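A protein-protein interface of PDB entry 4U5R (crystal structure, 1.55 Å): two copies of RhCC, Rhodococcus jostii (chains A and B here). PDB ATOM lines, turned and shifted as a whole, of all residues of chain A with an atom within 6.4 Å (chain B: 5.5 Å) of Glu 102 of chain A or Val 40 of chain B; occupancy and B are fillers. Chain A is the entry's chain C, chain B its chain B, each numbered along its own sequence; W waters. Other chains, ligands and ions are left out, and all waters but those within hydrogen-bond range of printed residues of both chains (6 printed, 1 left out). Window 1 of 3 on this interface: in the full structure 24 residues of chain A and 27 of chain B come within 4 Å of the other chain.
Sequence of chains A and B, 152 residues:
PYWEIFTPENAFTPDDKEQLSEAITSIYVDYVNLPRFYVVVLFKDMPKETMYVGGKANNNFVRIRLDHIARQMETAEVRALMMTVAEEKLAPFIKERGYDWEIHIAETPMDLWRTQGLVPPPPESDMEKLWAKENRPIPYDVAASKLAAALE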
ATOM      1  N   MET A  51       8.098   0.034 -27.053  1.00  0.00           N
ATOM      2  CA  MET A  51       8.676   1.359 -27.273  1.00  0.00           C
ATOM      3  C   MET A  51      10.024   1.204 -27.953  1.00  0.00           C
ATOM      4  O   MET A  51      10.974   0.660 -27.377  1.00  0.00           O
ATOM      5  CB  MET A  51       8.832   2.131 -25.949  1.00  0.00           C
ATOM      6  CG  MET A  51       7.548   2.205 -25.128  1.00  0.00           C
ATOM      7  SD  MET A  51       7.671   3.095 -23.557  1.00  0.00           S
ATOM      8  CE  MET A  51       7.723   4.803 -24.110  1.00  0.00           C
ATOM      9  N   TYR A  52      10.109   1.663 -29.192  1.00  0.00           N
ATOM     10  CA  TYR A  52      11.340   1.512 -29.949  1.00  0.00           C
ATOM     11  C   TYR A  52      12.029   2.851 -30.198  1.00  0.00           C
ATOM     12  O   TYR A  52      11.450   3.782 -30.773  1.00  0.00           O
ATOM     13  CB  TYR A  52      11.050   0.778 -31.266  1.00  0.00           C
ATOM     14  CG  TYR A  52      10.808  -0.698 -31.030  1.00  0.00           C
ATOM     15  CD1 TYR A  52       9.613  -1.148 -30.477  1.00  0.00           C
ATOM     16  CD2 TYR A  52      11.786  -1.631 -31.344  1.00  0.00           C
ATOM     17  CE1 TYR A  52       9.400  -2.494 -30.232  1.00  0.00           C
ATOM     18  CE2 TYR A  52      11.584  -2.983 -31.103  1.00  0.00           C
ATOM     19  CZ  TYR A  52      10.390  -3.404 -30.556  1.00  0.00           C
ATOM     20  OH  TYR A  52      10.175  -4.742 -30.312  1.00  0.00           O
ATOM     21  N   VAL A  53      13.278   2.931 -29.743  1.00  0.00           N
ATOM     22  CA  VAL A  53      14.074   4.142 -29.853  1.00  0.00           C
ATOM     23  C   VAL A  53      15.236   3.901 -30.807  1.00  0.00           C
ATOM     24  O   VAL A  53      16.069   3.050 -30.544  1.00  0.00           O
ATOM     25  CB  VAL A  53      14.603   4.573 -28.470  1.00  0.00           C
ATOM     26  CG1 VAL A  53      15.485   5.820 -28.595  1.00  0.00           C
ATOM     27  CG2 VAL A  53      13.442   4.804 -27.506  1.00  0.00           C
ATOM     28  N   GLY A  54      15.297   4.630 -31.918  1.00  0.00           N
ATOM     29  CA  GLY A  54      16.351   4.388 -32.890  1.00  0.00           C
ATOM     30  C   GLY A  54      16.380   2.966 -33.436  1.00  0.00           C
ATOM     31  O   GLY A  54      17.452   2.451 -33.767  1.00  0.00           O
ATOM     32  N   PHE A  61      12.276   3.372 -20.759  1.00  0.00           N
ATOM     33  CA  PHE A  61      12.102   4.661 -21.431  1.00  0.00           C
ATOM     34  C   PHE A  61      10.724   5.237 -21.129  1.00  0.00           C
ATOM     35  O   PHE A  61       9.720   4.542 -21.262  1.00  0.00           O
ATOM     36  CB  PHE A  61      12.311   4.472 -22.938  1.00  0.00           C
ATOM     37  CG  PHE A  61      12.170   5.727 -23.769  1.00  0.00           C
ATOM     38  CD1 PHE A  61      13.005   6.807 -23.571  1.00  0.00           C
ATOM     39  CD2 PHE A  61      11.243   5.787 -24.803  1.00  0.00           C
ATOM     40  CE1 PHE A  61      12.899   7.956 -24.367  1.00  0.00           C
ATOM     41  CE2 PHE A  61      11.129   6.922 -25.591  1.00  0.00           C
ATOM     42  CZ  PHE A  61      11.960   8.007 -25.376  1.00  0.00           C
ATOM     43  N   VAL A  62      10.690   6.493 -20.685  1.00  0.00           N
ATOM     44  CA  VAL A  62       9.441   7.190 -20.413  1.00  0.00           C
ATOM     45  C   VAL A  62       9.251   8.280 -21.459  1.00  0.00           C
ATOM     46  O   VAL A  62      10.122   9.122 -21.625  1.00  0.00           O
ATOM     47  CB  VAL A  62       9.428   7.812 -19.003  1.00  0.00           C
ATOM     48  CG1 VAL A  62       8.185   8.686 -18.815  1.00  0.00           C
ATOM     49  CG2 VAL A  62       9.494   6.714 -17.914  1.00  0.00           C
ATOM     50  N   ARG A  63       8.144   8.237 -22.196  1.00  0.00           N
ATOM     51  CA  ARG A  63       7.869   9.238 -23.227  1.00  0.00           C
ATOM     52  C   ARG A  63       6.687  10.096 -22.818  1.00  0.00           C
ATOM     53  O   ARG A  63       5.621   9.570 -22.486  1.00  0.00           O
ATOM     54  CB  ARG A  63       7.603   8.559 -24.581  1.00  0.00           C
ATOM     55  CG  ARG A  63       7.560   9.522 -25.780  1.00  0.00           C
ATOM     56  CD  ARG A  63       8.877  10.289 -25.889  1.00  0.00           C
ATOM     57  NE  ARG A  63       9.034  11.023 -27.139  1.00  0.00           N
ATOM     58  CZ  ARG A  63       8.498  12.214 -27.404  1.00  0.00           C
ATOM     59  NH1 ARG A  63       7.678  12.795 -26.542  1.00  0.00           N
ATOM     60  NH2 ARG A  63       8.755  12.805 -28.564  1.00  0.00           N
ATOM     61  N   ILE A  64       6.877  11.417 -22.827  1.00  0.00           N
ATOM     62  CA  ILE A  64       5.832  12.343 -22.407  1.00  0.00           C
ATOM     63  C   ILE A  64       5.430  13.230 -23.570  1.00  0.00           C
ATOM     64  O   ILE A  64       6.278  13.738 -24.293  1.00  0.00           O
ATOM     65  CB  ILE A  64       6.296  13.218 -21.234  1.00  0.00           C
ATOM     66  CG1 ILE A  64       6.825  12.334 -20.105  1.00  0.00           C
ATOM     67  CG2 ILE A  64       5.174  14.155 -20.767  1.00  0.00           C
ATOM     68  CD1 ILE A  64       8.336  12.453 -19.905  1.00  0.00           C
ATOM     69  N   ARG A  65       4.128  13.396 -23.746  1.00  0.00           N
ATOM     70  CA  ARG A  65       3.606  14.314 -24.753  1.00  0.00           C
ATOM     71  C   ARG A  65       2.491  15.121 -24.148  1.00  0.00           C
ATOM     72  O   ARG A  65       1.657  14.574 -23.441  1.00  0.00           O
ATOM     73  CB  ARG A  65       3.088  13.567 -25.974  1.00  0.00           C
ATOM     74  CG  ARG A  65       2.682  14.489 -27.117  1.00  0.00           C
ATOM     75  CD  ARG A  65       1.901  13.713 -28.169  1.00  0.00           C
ATOM     76  NE  ARG A  65       1.630  14.568 -29.321  1.00  0.00           N
ATOM     77  CZ  ARG A  65       0.669  15.479 -29.367  1.00  0.00           C
ATOM     78  NH1 ARG A  65      -0.167  15.637 -28.341  1.00  0.00           N
ATOM     79  NH2 ARG A  65       0.541  16.228 -30.461  1.00  0.00           N
ATOM     80  N   GLU A  87      10.685  19.915 -16.539  1.00  0.00           N
ATOM     81  CA  GLU A  87      11.772  18.983 -16.236  1.00  0.00           C
ATOM     82  C   GLU A  87      12.067  18.935 -14.747  1.00  0.00           C
ATOM     83  O   GLU A  87      12.319  17.868 -14.208  1.00  0.00           O
ATOM     84  CB  GLU A  87      13.033  19.341 -17.022  1.00  0.00           C
ATOM     85  CG  GLU A  87      12.906  19.135 -18.533  1.00  0.00           C
ATOM     86  CD  GLU A  87      12.902  17.666 -18.953  1.00  0.00           C
ATOM     87  OE1 GLU A  87      13.073  16.771 -18.100  1.00  0.00           O
ATOM     88  OE2 GLU A  87      12.734  17.407 -20.155  1.00  0.00           O
ATOM     89  N   ASP A 100      15.451   6.635 -19.112  1.00  0.00           N
ATOM     90  CA  ASP A 100      15.666   7.538 -20.238  1.00  0.00           C
ATOM     91  C   ASP A 100      14.331   8.202 -20.494  1.00  0.00           C
ATOM     92  O   ASP A 100      13.303   7.590 -20.252  1.00  0.00           O
ATOM     93  CB  ASP A 100      16.122   6.793 -21.492  1.00  0.00           C
ATOM     94  CG  ASP A 100      17.466   6.105 -21.316  1.00  0.00           C
ATOM     95  OD1 ASP A 100      18.336   6.644 -20.595  1.00  0.00           O
ATOM     96  OD2 ASP A 100      17.636   5.018 -21.916  1.00  0.00           O
ATOM     97  N   TRP A 101      14.315   9.444 -20.967  1.00  0.00           N
ATOM     98  CA  TRP A 101      13.027  10.104 -21.183  1.00  0.00           C
ATOM     99  C   TRP A 101      13.099  11.203 -22.225  1.00  0.00           C
ATOM    100  O   TRP A 101      14.161  11.723 -22.552  1.00  0.00           O
ATOM    101  CB  TRP A 101      12.451  10.658 -19.850  1.00  0.00           C
ATOM    102  CG  TRP A 101      13.034  11.957 -19.380  1.00  0.00           C
ATOM    103  CD1 TRP A 101      12.439  13.194 -19.387  1.00  0.00           C
ATOM    104  CD2 TRP A 101      14.327  12.135 -18.829  1.00  0.00           C
ATOM    105  NE1 TRP A 101      13.306  14.136 -18.868  1.00  0.00           N
ATOM    106  CE2 TRP A 101      14.476  13.509 -18.520  1.00  0.00           C
ATOM    107  CE3 TRP A 101      15.377  11.259 -18.543  1.00  0.00           C
ATOM    108  CZ2 TRP A 101      15.646  14.023 -17.959  1.00  0.00           C
ATOM    109  CZ3 TRP A 101      16.540  11.773 -17.995  1.00  0.00           C
ATOM    110  CH2 TRP A 101      16.665  13.140 -17.715  1.00  0.00           C
ATOM    111  N   GLU A 102      11.935  11.542 -22.760  1.00  0.00           N
ATOM    112  CA  GLU A 102      11.817  12.593 -23.757  1.00  0.00           C
ATOM    113  C   GLU A 102      10.432  13.209 -23.650  1.00  0.00           C
ATOM    114  O   GLU A 102       9.473  12.505 -23.332  1.00  0.00           O
ATOM    115  CB  GLU A 102      12.071  12.021 -25.149  1.00  0.00           C
ATOM    116  CG  GLU A 102      12.005  13.041 -26.265  1.00  0.00           C
ATOM    117  CD  GLU A 102      12.273  12.412 -27.618  1.00  0.00           C
ATOM    118  OE1 GLU A 102      12.012  11.208 -27.790  1.00  0.00           O
ATOM    119  OE2 GLU A 102      12.761  13.125 -28.511  1.00  0.00           O
ATOM    120  N   ILE A 103      10.325  14.510 -23.930  1.00  0.00           N
ATOM    121  CA  ILE A 103       9.074  15.249 -23.779  1.00  0.00           C
ATOM    122  C   ILE A 103       8.898  16.264 -24.897  1.00  0.00           C
ATOM    123  O   ILE A 103       9.865  16.886 -25.330  1.00  0.00           O
ATOM    124  CB  ILE A 103       9.019  15.984 -22.420  1.00  0.00           C
ATOM    125  CG1 ILE A 103       7.671  16.690 -22.251  1.00  0.00           C
ATOM    126  CG2 ILE A 103      10.168  17.012 -22.304  1.00  0.00           C
ATOM    127  CD1 ILE A 103       7.480  17.279 -20.840  1.00  0.00           C
ATOM    128  N   HIS A 104       7.674  16.404 -25.396  1.00  0.00           N
ATOM    129  CA  HIS A 104       7.346  17.532 -26.272  1.00  0.00           C
ATOM    130  C   HIS A 104       5.919  18.013 -26.090  1.00  0.00           C
ATOM    131  O   HIS A 104       5.056  17.295 -25.566  1.00  0.00           O
ATOM    132  CB  HIS A 104       7.624  17.208 -27.756  1.00  0.00           C
ATOM    133  CG  HIS A 104       6.633  16.295 -28.422  1.00  0.00           C
ATOM    134  ND1 HIS A 104       6.561  14.946 -28.147  1.00  0.00           N
ATOM    135  CD2 HIS A 104       5.767  16.516 -29.443  1.00  0.00           C
ATOM    136  CE1 HIS A 104       5.663  14.383 -28.936  1.00  0.00           C
ATOM    137  NE2 HIS A 104       5.163  15.315 -29.731  1.00  0.00           N
ATOM    138  N   PRO B   1      11.381  12.411 -34.288  1.00  0.00           N
ATOM    139  CA  PRO B   1      10.023  12.073 -34.717  1.00  0.00           C
ATOM    140  C   PRO B   1       9.338  11.167 -33.714  1.00  0.00           C
ATOM    141  O   PRO B   1       9.971  10.335 -33.063  1.00  0.00           O
ATOM    142  CB  PRO B   1      10.243  11.357 -36.053  1.00  0.00           C
ATOM    143  CG  PRO B   1      11.584  11.837 -36.512  1.00  0.00           C
ATOM    144  CD  PRO B   1      12.385  11.986 -35.273  1.00  0.00           C
ATOM    145  N   TYR B   2       8.032  11.332 -33.609  1.00  0.00           N
ATOM    146  CA  TYR B   2       7.247  10.582 -32.647  1.00  0.00           C
ATOM    147  C   TYR B   2       6.172   9.798 -33.373  1.00  0.00           C
ATOM    148  O   TYR B   2       5.219  10.391 -33.857  1.00  0.00           O
ATOM    149  CB  TYR B   2       6.643  11.564 -31.647  1.00  0.00           C
ATOM    150  CG  TYR B   2       5.618  11.015 -30.705  1.00  0.00           C
ATOM    151  CD1 TYR B   2       6.001  10.305 -29.577  1.00  0.00           C
ATOM    152  CD2 TYR B   2       4.266  11.269 -30.903  1.00  0.00           C
ATOM    153  CE1 TYR B   2       5.048   9.831 -28.683  1.00  0.00           C
ATOM    154  CE2 TYR B   2       3.309  10.794 -30.026  1.00  0.00           C
ATOM    155  CZ  TYR B   2       3.715  10.072 -28.915  1.00  0.00           C
ATOM    156  OH  TYR B   2       2.792   9.600 -28.010  1.00  0.00           O
ATOM    157  N   TRP B   3       6.328   8.478 -33.458  1.00  0.00           N
ATOM    158  CA  TRP B   3       5.373   7.638 -34.188  1.00  0.00           C
ATOM    159  C   TRP B   3       4.517   6.788 -33.268  1.00  0.00           C
ATOM    160  O   TRP B   3       5.019   6.167 -32.328  1.00  0.00           O
ATOM    161  CB  TRP B   3       6.092   6.693 -35.151  1.00  0.00           C
ATOM    162  CG  TRP B   3       6.680   7.294 -36.375  1.00  0.00           C
ATOM    163  CD1 TRP B   3       7.614   8.296 -36.448  1.00  0.00           C
ATOM    164  CD2 TRP B   3       6.428   6.877 -37.715  1.00  0.00           C
ATOM    165  NE1 TRP B   3       7.926   8.547 -37.765  1.00  0.00           N
ATOM    166  CE2 TRP B   3       7.213   7.686 -38.559  1.00  0.00           C
ATOM    167  CE3 TRP B   3       5.588   5.914 -38.285  1.00  0.00           C
ATOM    168  CZ2 TRP B   3       7.196   7.553 -39.950  1.00  0.00           C
ATOM    169  CZ3 TRP B   3       5.578   5.775 -39.671  1.00  0.00           C
ATOM    170  CH2 TRP B   3       6.368   6.601 -40.484  1.00  0.00           C
ATOM    171  N   GLU B   4       3.226   6.745 -33.565  1.00  0.00           N
ATOM    172  CA  GLU B   4       2.317   5.815 -32.929  1.00  0.00           C
ATOM    173  C   GLU B   4       1.773   4.864 -33.966  1.00  0.00           C
ATOM    174  O   GLU B   4       1.232   5.313 -34.965  1.00  0.00           O
ATOM    175  CB  GLU B   4       1.161   6.547 -32.290  1.00  0.00           C
ATOM    176  CG  GLU B   4       1.492   7.347 -31.067  1.00  0.00           C
ATOM    177  CD  GLU B   4       0.287   8.143 -30.623  1.00  0.00           C
ATOM    178  OE1 GLU B   4      -0.167   9.009 -31.404  1.00  0.00           O
ATOM    179  OE2 GLU B   4      -0.238   7.867 -29.528  1.00  0.00           O
ATOM    180  N   PHE B  37      18.403   8.009 -32.239  1.00  0.00           N
ATOM    181  CA  PHE B  37      17.565   7.940 -31.049  1.00  0.00           C
ATOM    182  C   PHE B  37      16.454   9.004 -31.001  1.00  0.00           C
ATOM    183  O   PHE B  37      15.571   8.892 -30.152  1.00  0.00           O
ATOM    184  CB  PHE B  37      18.408   8.028 -29.766  1.00  0.00           C
ATOM    185  CG  PHE B  37      19.040   9.370 -29.539  1.00  0.00           C
ATOM    186  CD1 PHE B  37      18.379  10.362 -28.831  1.00  0.00           C
ATOM    187  CD2 PHE B  37      20.318   9.616 -29.999  1.00  0.00           C
ATOM    188  CE1 PHE B  37      18.979  11.592 -28.624  1.00  0.00           C
ATOM    189  CE2 PHE B  37      20.922  10.846 -29.790  1.00  0.00           C
ATOM    190  CZ  PHE B  37      20.247  11.828 -29.094  1.00  0.00           C
ATOM    191  N   TYR B  38      16.501  10.016 -31.879  1.00  0.00           N
ATOM    192  CA  TYR B  38      15.366  10.941 -32.062  1.00  0.00           C
ATOM    193  C   TYR B  38      14.105  10.202 -32.506  1.00  0.00           C
ATOM    194  O   TYR B  38      12.990  10.642 -32.208  1.00  0.00           O
ATOM    195  CB  TYR B  38      15.650  12.032 -33.108  1.00  0.00           C
ATOM    196  CG  TYR B  38      16.525  13.189 -32.681  1.00  0.00           C
ATOM    197  CD1 TYR B  38      17.178  13.187 -31.460  1.00  0.00           C
ATOM    198  CD2 TYR B  38      16.691  14.282 -33.516  1.00  0.00           C
ATOM    199  CE1 TYR B  38      17.991  14.245 -31.087  1.00  0.00           C
ATOM    200  CE2 TYR B  38      17.489  15.349 -33.150  1.00  0.00           C
ATOM    201  CZ  TYR B  38      18.135  15.318 -31.940  1.00  0.00           C
ATOM    202  OH  TYR B  38      18.942  16.369 -31.588  1.00  0.00           O
ATOM    203  N   VAL B  39      14.278   9.096 -33.229  1.00  0.00           N
ATOM    204  CA  VAL B  39      13.133   8.391 -33.812  1.00  0.00           C
ATOM    205  C   VAL B  39      12.516   7.404 -32.816  1.00  0.00           C
ATOM    206  O   VAL B  39      13.083   6.348 -32.517  1.00  0.00           O
ATOM    207  CB  VAL B  39      13.539   7.647 -35.107  1.00  0.00           C
ATOM    208  CG1 VAL B  39      12.307   7.182 -35.860  1.00  0.00           C
ATOM    209  CG2 VAL B  39      14.358   8.556 -36.004  1.00  0.00           C
ATOM    210  N   VAL B  40      11.334   7.765 -32.331  1.00  0.00           N
ATOM    211  CA  VAL B  40      10.613   6.963 -31.347  1.00  0.00           C
ATOM    212  C   VAL B  40       9.373   6.366 -32.018  1.00  0.00           C
ATOM    213  O   VAL B  40       8.585   7.078 -32.664  1.00  0.00           O
ATOM    214  CB  VAL B  40      10.215   7.810 -30.115  1.00  0.00           C
ATOM    215  CG1 VAL B  40       9.319   7.017 -29.177  1.00  0.00           C
ATOM    216  CG2 VAL B  40      11.464   8.329 -29.387  1.00  0.00           C
ATOM    217  N   VAL B  41       9.209   5.055 -31.887  1.00  0.00           N
ATOM    218  CA  VAL B  41       8.038   4.373 -32.430  1.00  0.00           C
ATOM    219  C   VAL B  41       7.329   3.607 -31.313  1.00  0.00           C
ATOM    220  O   VAL B  41       7.895   2.697 -30.672  1.00  0.00           O
ATOM    221  CB  VAL B  41       8.399   3.400 -33.576  1.00  0.00           C
ATOM    222  CG1 VAL B  41       7.125   2.764 -34.122  1.00  0.00           C
ATOM    223  CG2 VAL B  41       9.127   4.107 -34.701  1.00  0.00           C
ATOM    224  N   LEU B  42       6.081   3.973 -31.065  1.00  0.00           N
ATOM    225  CA  LEU B  42       5.309   3.324 -30.015  1.00  0.00           C
ATOM    226  C   LEU B  42       4.279   2.391 -30.650  1.00  0.00           C
ATOM    227  O   LEU B  42       3.406   2.847 -31.393  1.00  0.00           O
ATOM    228  CB  LEU B  42       4.615   4.365 -29.116  1.00  0.00           C
ATOM    229  CG  LEU B  42       5.477   5.507 -28.555  1.00  0.00           C
ATOM    230  CD1 LEU B  42       4.651   6.412 -27.650  1.00  0.00           C
ATOM    231  CD2 LEU B  42       6.682   4.952 -27.803  1.00  0.00           C
ATOM    232  N   ILE B  69       9.027  17.049 -35.007  1.00  0.00           N
ATOM    233  CA  ILE B  69       9.438  18.062 -34.045  1.00  0.00           C
ATOM    234  C   ILE B  69      10.724  18.756 -34.444  1.00  0.00           C
ATOM    235  O   ILE B  69      10.839  19.971 -34.318  1.00  0.00           O
ATOM    236  CB  ILE B  69       9.637  17.441 -32.655  1.00  0.00           C
ATOM    237  CG1 ILE B  69       8.453  16.530 -32.321  1.00  0.00           C
ATOM    238  CG2 ILE B  69       9.821  18.535 -31.608  1.00  0.00           C
ATOM    239  CD1 ILE B  69       8.779  15.426 -31.290  1.00  0.00           C
ATOM    240  N   TRP B 113      10.502  21.039 -26.712  1.00  0.00           N
ATOM    241  CA  TRP B 113      10.958  19.674 -26.883  1.00  0.00           C
ATOM    242  C   TRP B 113      12.272  19.494 -26.145  1.00  0.00           C
ATOM    243  O   TRP B 113      13.191  20.273 -26.328  1.00  0.00           O
ATOM    244  CB  TRP B 113      11.105  19.378 -28.381  1.00  0.00           C
ATOM    245  CG  TRP B 113      11.843  18.119 -28.725  1.00  0.00           C
ATOM    246  CD1 TRP B 113      11.714  16.887 -28.133  1.00  0.00           C
ATOM    247  CD2 TRP B 113      12.833  17.966 -29.750  1.00  0.00           C
ATOM    248  NE1 TRP B 113      12.551  15.983 -28.742  1.00  0.00           N
ATOM    249  CE2 TRP B 113      13.249  16.621 -29.734  1.00  0.00           C
ATOM    250  CE3 TRP B 113      13.400  18.840 -30.684  1.00  0.00           C
ATOM    251  CZ2 TRP B 113      14.222  16.128 -30.606  1.00  0.00           C
ATOM    252  CZ3 TRP B 113      14.363  18.351 -31.548  1.00  0.00           C
ATOM    253  CH2 TRP B 113      14.761  17.005 -31.507  1.00  0.00           C
ATOM    254  N   ARG B 114      12.359  18.482 -25.291  1.00  0.00           N
ATOM    255  CA  ARG B 114      13.609  18.178 -24.620  1.00  0.00           C
ATOM    256  C   ARG B 114      13.820  16.680 -24.706  1.00  0.00           C
ATOM    257  O   ARG B 114      12.858  15.908 -24.673  1.00  0.00           O
ATOM    258  CB  ARG B 114      13.591  18.630 -23.148  1.00  0.00           C
ATOM    259  CG  ARG B 114      13.310  20.118 -22.925  1.00  0.00           C
ATOM    260  CD  ARG B 114      14.528  20.944 -23.325  1.00  0.00           C
ATOM    261  NE  ARG B 114      14.383  22.362 -23.011  1.00  0.00           N
ATOM    262  CZ  ARG B 114      13.942  23.287 -23.862  1.00  0.00           C
ATOM    263  NH1 ARG B 114      13.569  22.959 -25.101  1.00  0.00           N
ATOM    264  NH2 ARG B 114      13.861  24.553 -23.464  1.00  0.00           N
ATOM    265  N   THR B 115      15.068  16.251 -24.805  1.00  0.00           N
ATOM    266  CA  THR B 115      15.353  14.830 -24.699  1.00  0.00           C
ATOM    267  C   THR B 115      16.432  14.619 -23.633  1.00  0.00           C
ATOM    268  O   THR B 115      17.443  15.312 -23.621  1.00  0.00           O
ATOM    269  CB  THR B 115      15.757  14.223 -26.055  1.00  0.00           C
ATOM    270  OG1 THR B 115      15.857  12.790 -25.921  1.00  0.00           O
ATOM    271  CG2 THR B 115      17.066  14.836 -26.581  1.00  0.00           C
ATOM    272  N   GLN B 116      16.184  13.678 -22.725  1.00  0.00           N
ATOM    273  CA  GLN B 116      16.987  13.490 -21.504  1.00  0.00           C
ATOM    274  C   GLN B 116      17.199  14.812 -20.743  1.00  0.00           C
ATOM    275  O   GLN B 116      18.258  15.037 -20.134  1.00  0.00           O
ATOM    276  CB  GLN B 116      18.338  12.845 -21.838  1.00  0.00           C
ATOM    277  CG  GLN B 116      18.847  11.843 -20.800  1.00  0.00           C
ATOM    278  CD  GLN B 116      18.180  10.474 -20.872  1.00  0.00           C
ATOM    279  OE1 GLN B 116      17.187  10.272 -21.570  1.00  0.00           O
ATOM    280  NE2 GLN B 116      18.746   9.520 -20.157  1.00  0.00           N
HETATM  281  O   HOH W   1      12.441  12.946 -31.308  1.00  0.00           O
HETATM  282  O   HOH W   2      13.478  15.317 -21.713  1.00  0.00           O
HETATM  283  O   HOH W   3      16.635  10.584 -24.253  1.00  0.00           O
HETATM  284  O   HOH W   4      12.579   3.693 -33.522  1.00  0.00           O
HETATM  285  O   HOH W   5      14.227   9.830 -27.907  1.00  0.00           O
HETATM  286  O   HOH W   6      15.444  11.999 -28.418  1.00  0.00           O
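N of Arg 114 of chain B is in hydrogen-bond range of O of Ile 103 of chain A, 3.0 Å away.
The side-chain amide nitrogen (NE2) of Gln 116 of chain B lies within hydrogen-bond range of the side-chain carboxylate (OD1) of Asp 100 of chain A, at 2.9 Å.
O of Val 39 of chain B sits at hydrogen-bond distance from N of Gly 54 of chain A.
N of Val 41 of chain B sits at hydrogen-bond distance from O of Tyr 52 of chain A (2.8 Å).
The backbone NH (N) of Gln 116 of chain B lies within hydrogen-bond range of the backbone carbonyl oxygen (O) of Trp 101 of chain A (2.8 Å).
NE1 of Trp 113 of chain B is in hydrogen-bond range of OE2 of Glu 102 of chain A (2.9 Å).
The backbone carbonyl oxygen (O) of Trp 3 of chain B is in hydrogen-bond range of the backbone NH (N) of Leu 42 of chain B (2.7 Å).
OE1 of Glu 87 of chain A sits at hydrogen-bond distance from NE1 of Trp 101 of chain A, at 2.8 Å.
The backbone carbonyl oxygen (O) of Pro 1 of chain B lies within hydrogen-bond range of the backbone NH (N) of Val 40 of chain B, at 3.0 Å.
The backbone NH of Trp 3 of chain B lies within hydrogen-bond range of the backbone carbonyl oxygen of Val 40 of chain B (2.8 Å).
The backbone NH (N) of Glu 102 of chain A lies within hydrogen-bond range of the backbone carbonyl oxygen (O) of Val 62 of chain A, 3.2 Å away.
O of Asp 100 of chain A is in hydrogen-bond range of N of Val 62 of chain A, at 2.9 Å.
Among the printed residues, pairs that only touch across the chains: Met 51 of chain A with Val 41 of chain B (3.7 Å), Met 51 of chain A with Leu 42 of chain B (3.8 Å), Tyr 52 of chain A with Val 39 of chain B (3.5 Å), Tyr 52 of chain A with Val 40 of chain B (3.3 Å), Val 53 of chain A with Phe 37 of chain B (3.4 Å), Val 53 of chain A with Val 39 of chain B (3.6 Å), Arg 63 of chain A with Tyr 2 of chain B (3.8 Å), Arg 63 of chain A with Ile 69 of chain B (3.8 Å), Arg 65 of chain A with Tyr 2 of chain B (3.7 Å), Glu 87 of chain A with Arg 114 of chain B (3.3 Å), Trp 101 of chain A with Thr 115 of chain B (3.8 Å), Glu 102 of chain A with Val 40 of chain B (3.3 Å), Glu 102 of chain A with Arg 114 of chain B (3.4 Å), Glu 102 of chain A with Thr 115 of chain B (3.9 Å), Ile 103 of chain A with Trp 113 of chain B (3.4 Å), His 104 of chain A with Tyr 2 of chain B (3.8 Å) and His 104 of chain A with Ile 69 of chain B (3.7 Å).
Of the printed residues of chain B, Glu 102 of chain A touches Val 40, Trp 113, Arg 114 and Thr 115.
Of the printed residues of chain A, Val 40 of chain B touches Tyr 52 (3.3 Å) and Glu 102 (3.3 Å).
Of the printed residues of chain B, His 104 of chain A touches Tyr 2 and Ile 69.
Of the printed residues of chain A, Thr 115 of chain B touches Trp 101 and Glu 102.
Of the printed residues of chain A, Trp 113 of chain B touches Glu 102 and Ile 103.
Printed residues of chain A within 4 Å of Ile 69 of chain B: Arg 63 and His 104.
The nearest printed residue of chain A that does not touch Val 40 of chain B is Phe 61 of chain A (4.02 Å).
Printed residues of chain A that touch a printed residue of chain B: Met 51, Tyr 52, Val 53, Gly 54, Arg 63, Arg 65, Glu 87, Asp 100, Trp 101, Glu 102, Ile 103 and His 104.
Along chain A the printed residues that touch a printed residue of chain B span positions 51 to 104.
Among the printed residues, 23 pairs touch across the chains.
No position is printed for both chains.
Water W1 bridges the backbone carbonyl oxygen of Tyr 38 of chain B (2.5 Å) and the side-chain carboxylate of Glu 102 of chain A (2.8 Å).
Water W5 lies within hydrogen-bond range of the side-chain carboxylate of Glu 102 of chain A (2.6 Å) and the backbone carbonyl oxygen of Phe 37 of chain B (2.8 Å).
Water W6 lies within hydrogen-bond range of the side-chain hydroxyl of Thr 115 of chain B (2.7 Å) and the side-chain carboxylate of Glu 102 of chain A (2.9 Å).
Water W2 lies within hydrogen-bond range of the side-chain carboxylate of Glu 87 of chain A (2.7 Å), the backbone carbonyl oxygen of Arg 114 of chain B (3.1 Å), the indole nitrogen of Trp 101 of chain A (3.1 Å) and the backbone NH of Gln 116 of chain B (3.3 Å).
Water W3 lies within hydrogen-bond range of OE1 of Gln 116 of chain B (2.8 Å), OG1 of Thr 115 of chain B (2.9 Å) and O of Trp 101 of chain A (3.2 Å).
Water W4 lies within hydrogen-bond range of the backbone carbonyl oxygen of Val 39 of chain B (2.9 Å), the backbone carbonyl oxygen of Tyr 52 of chain A (3.0 Å) and the backbone NH of Gly 54 of chain A (3.3 Å).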
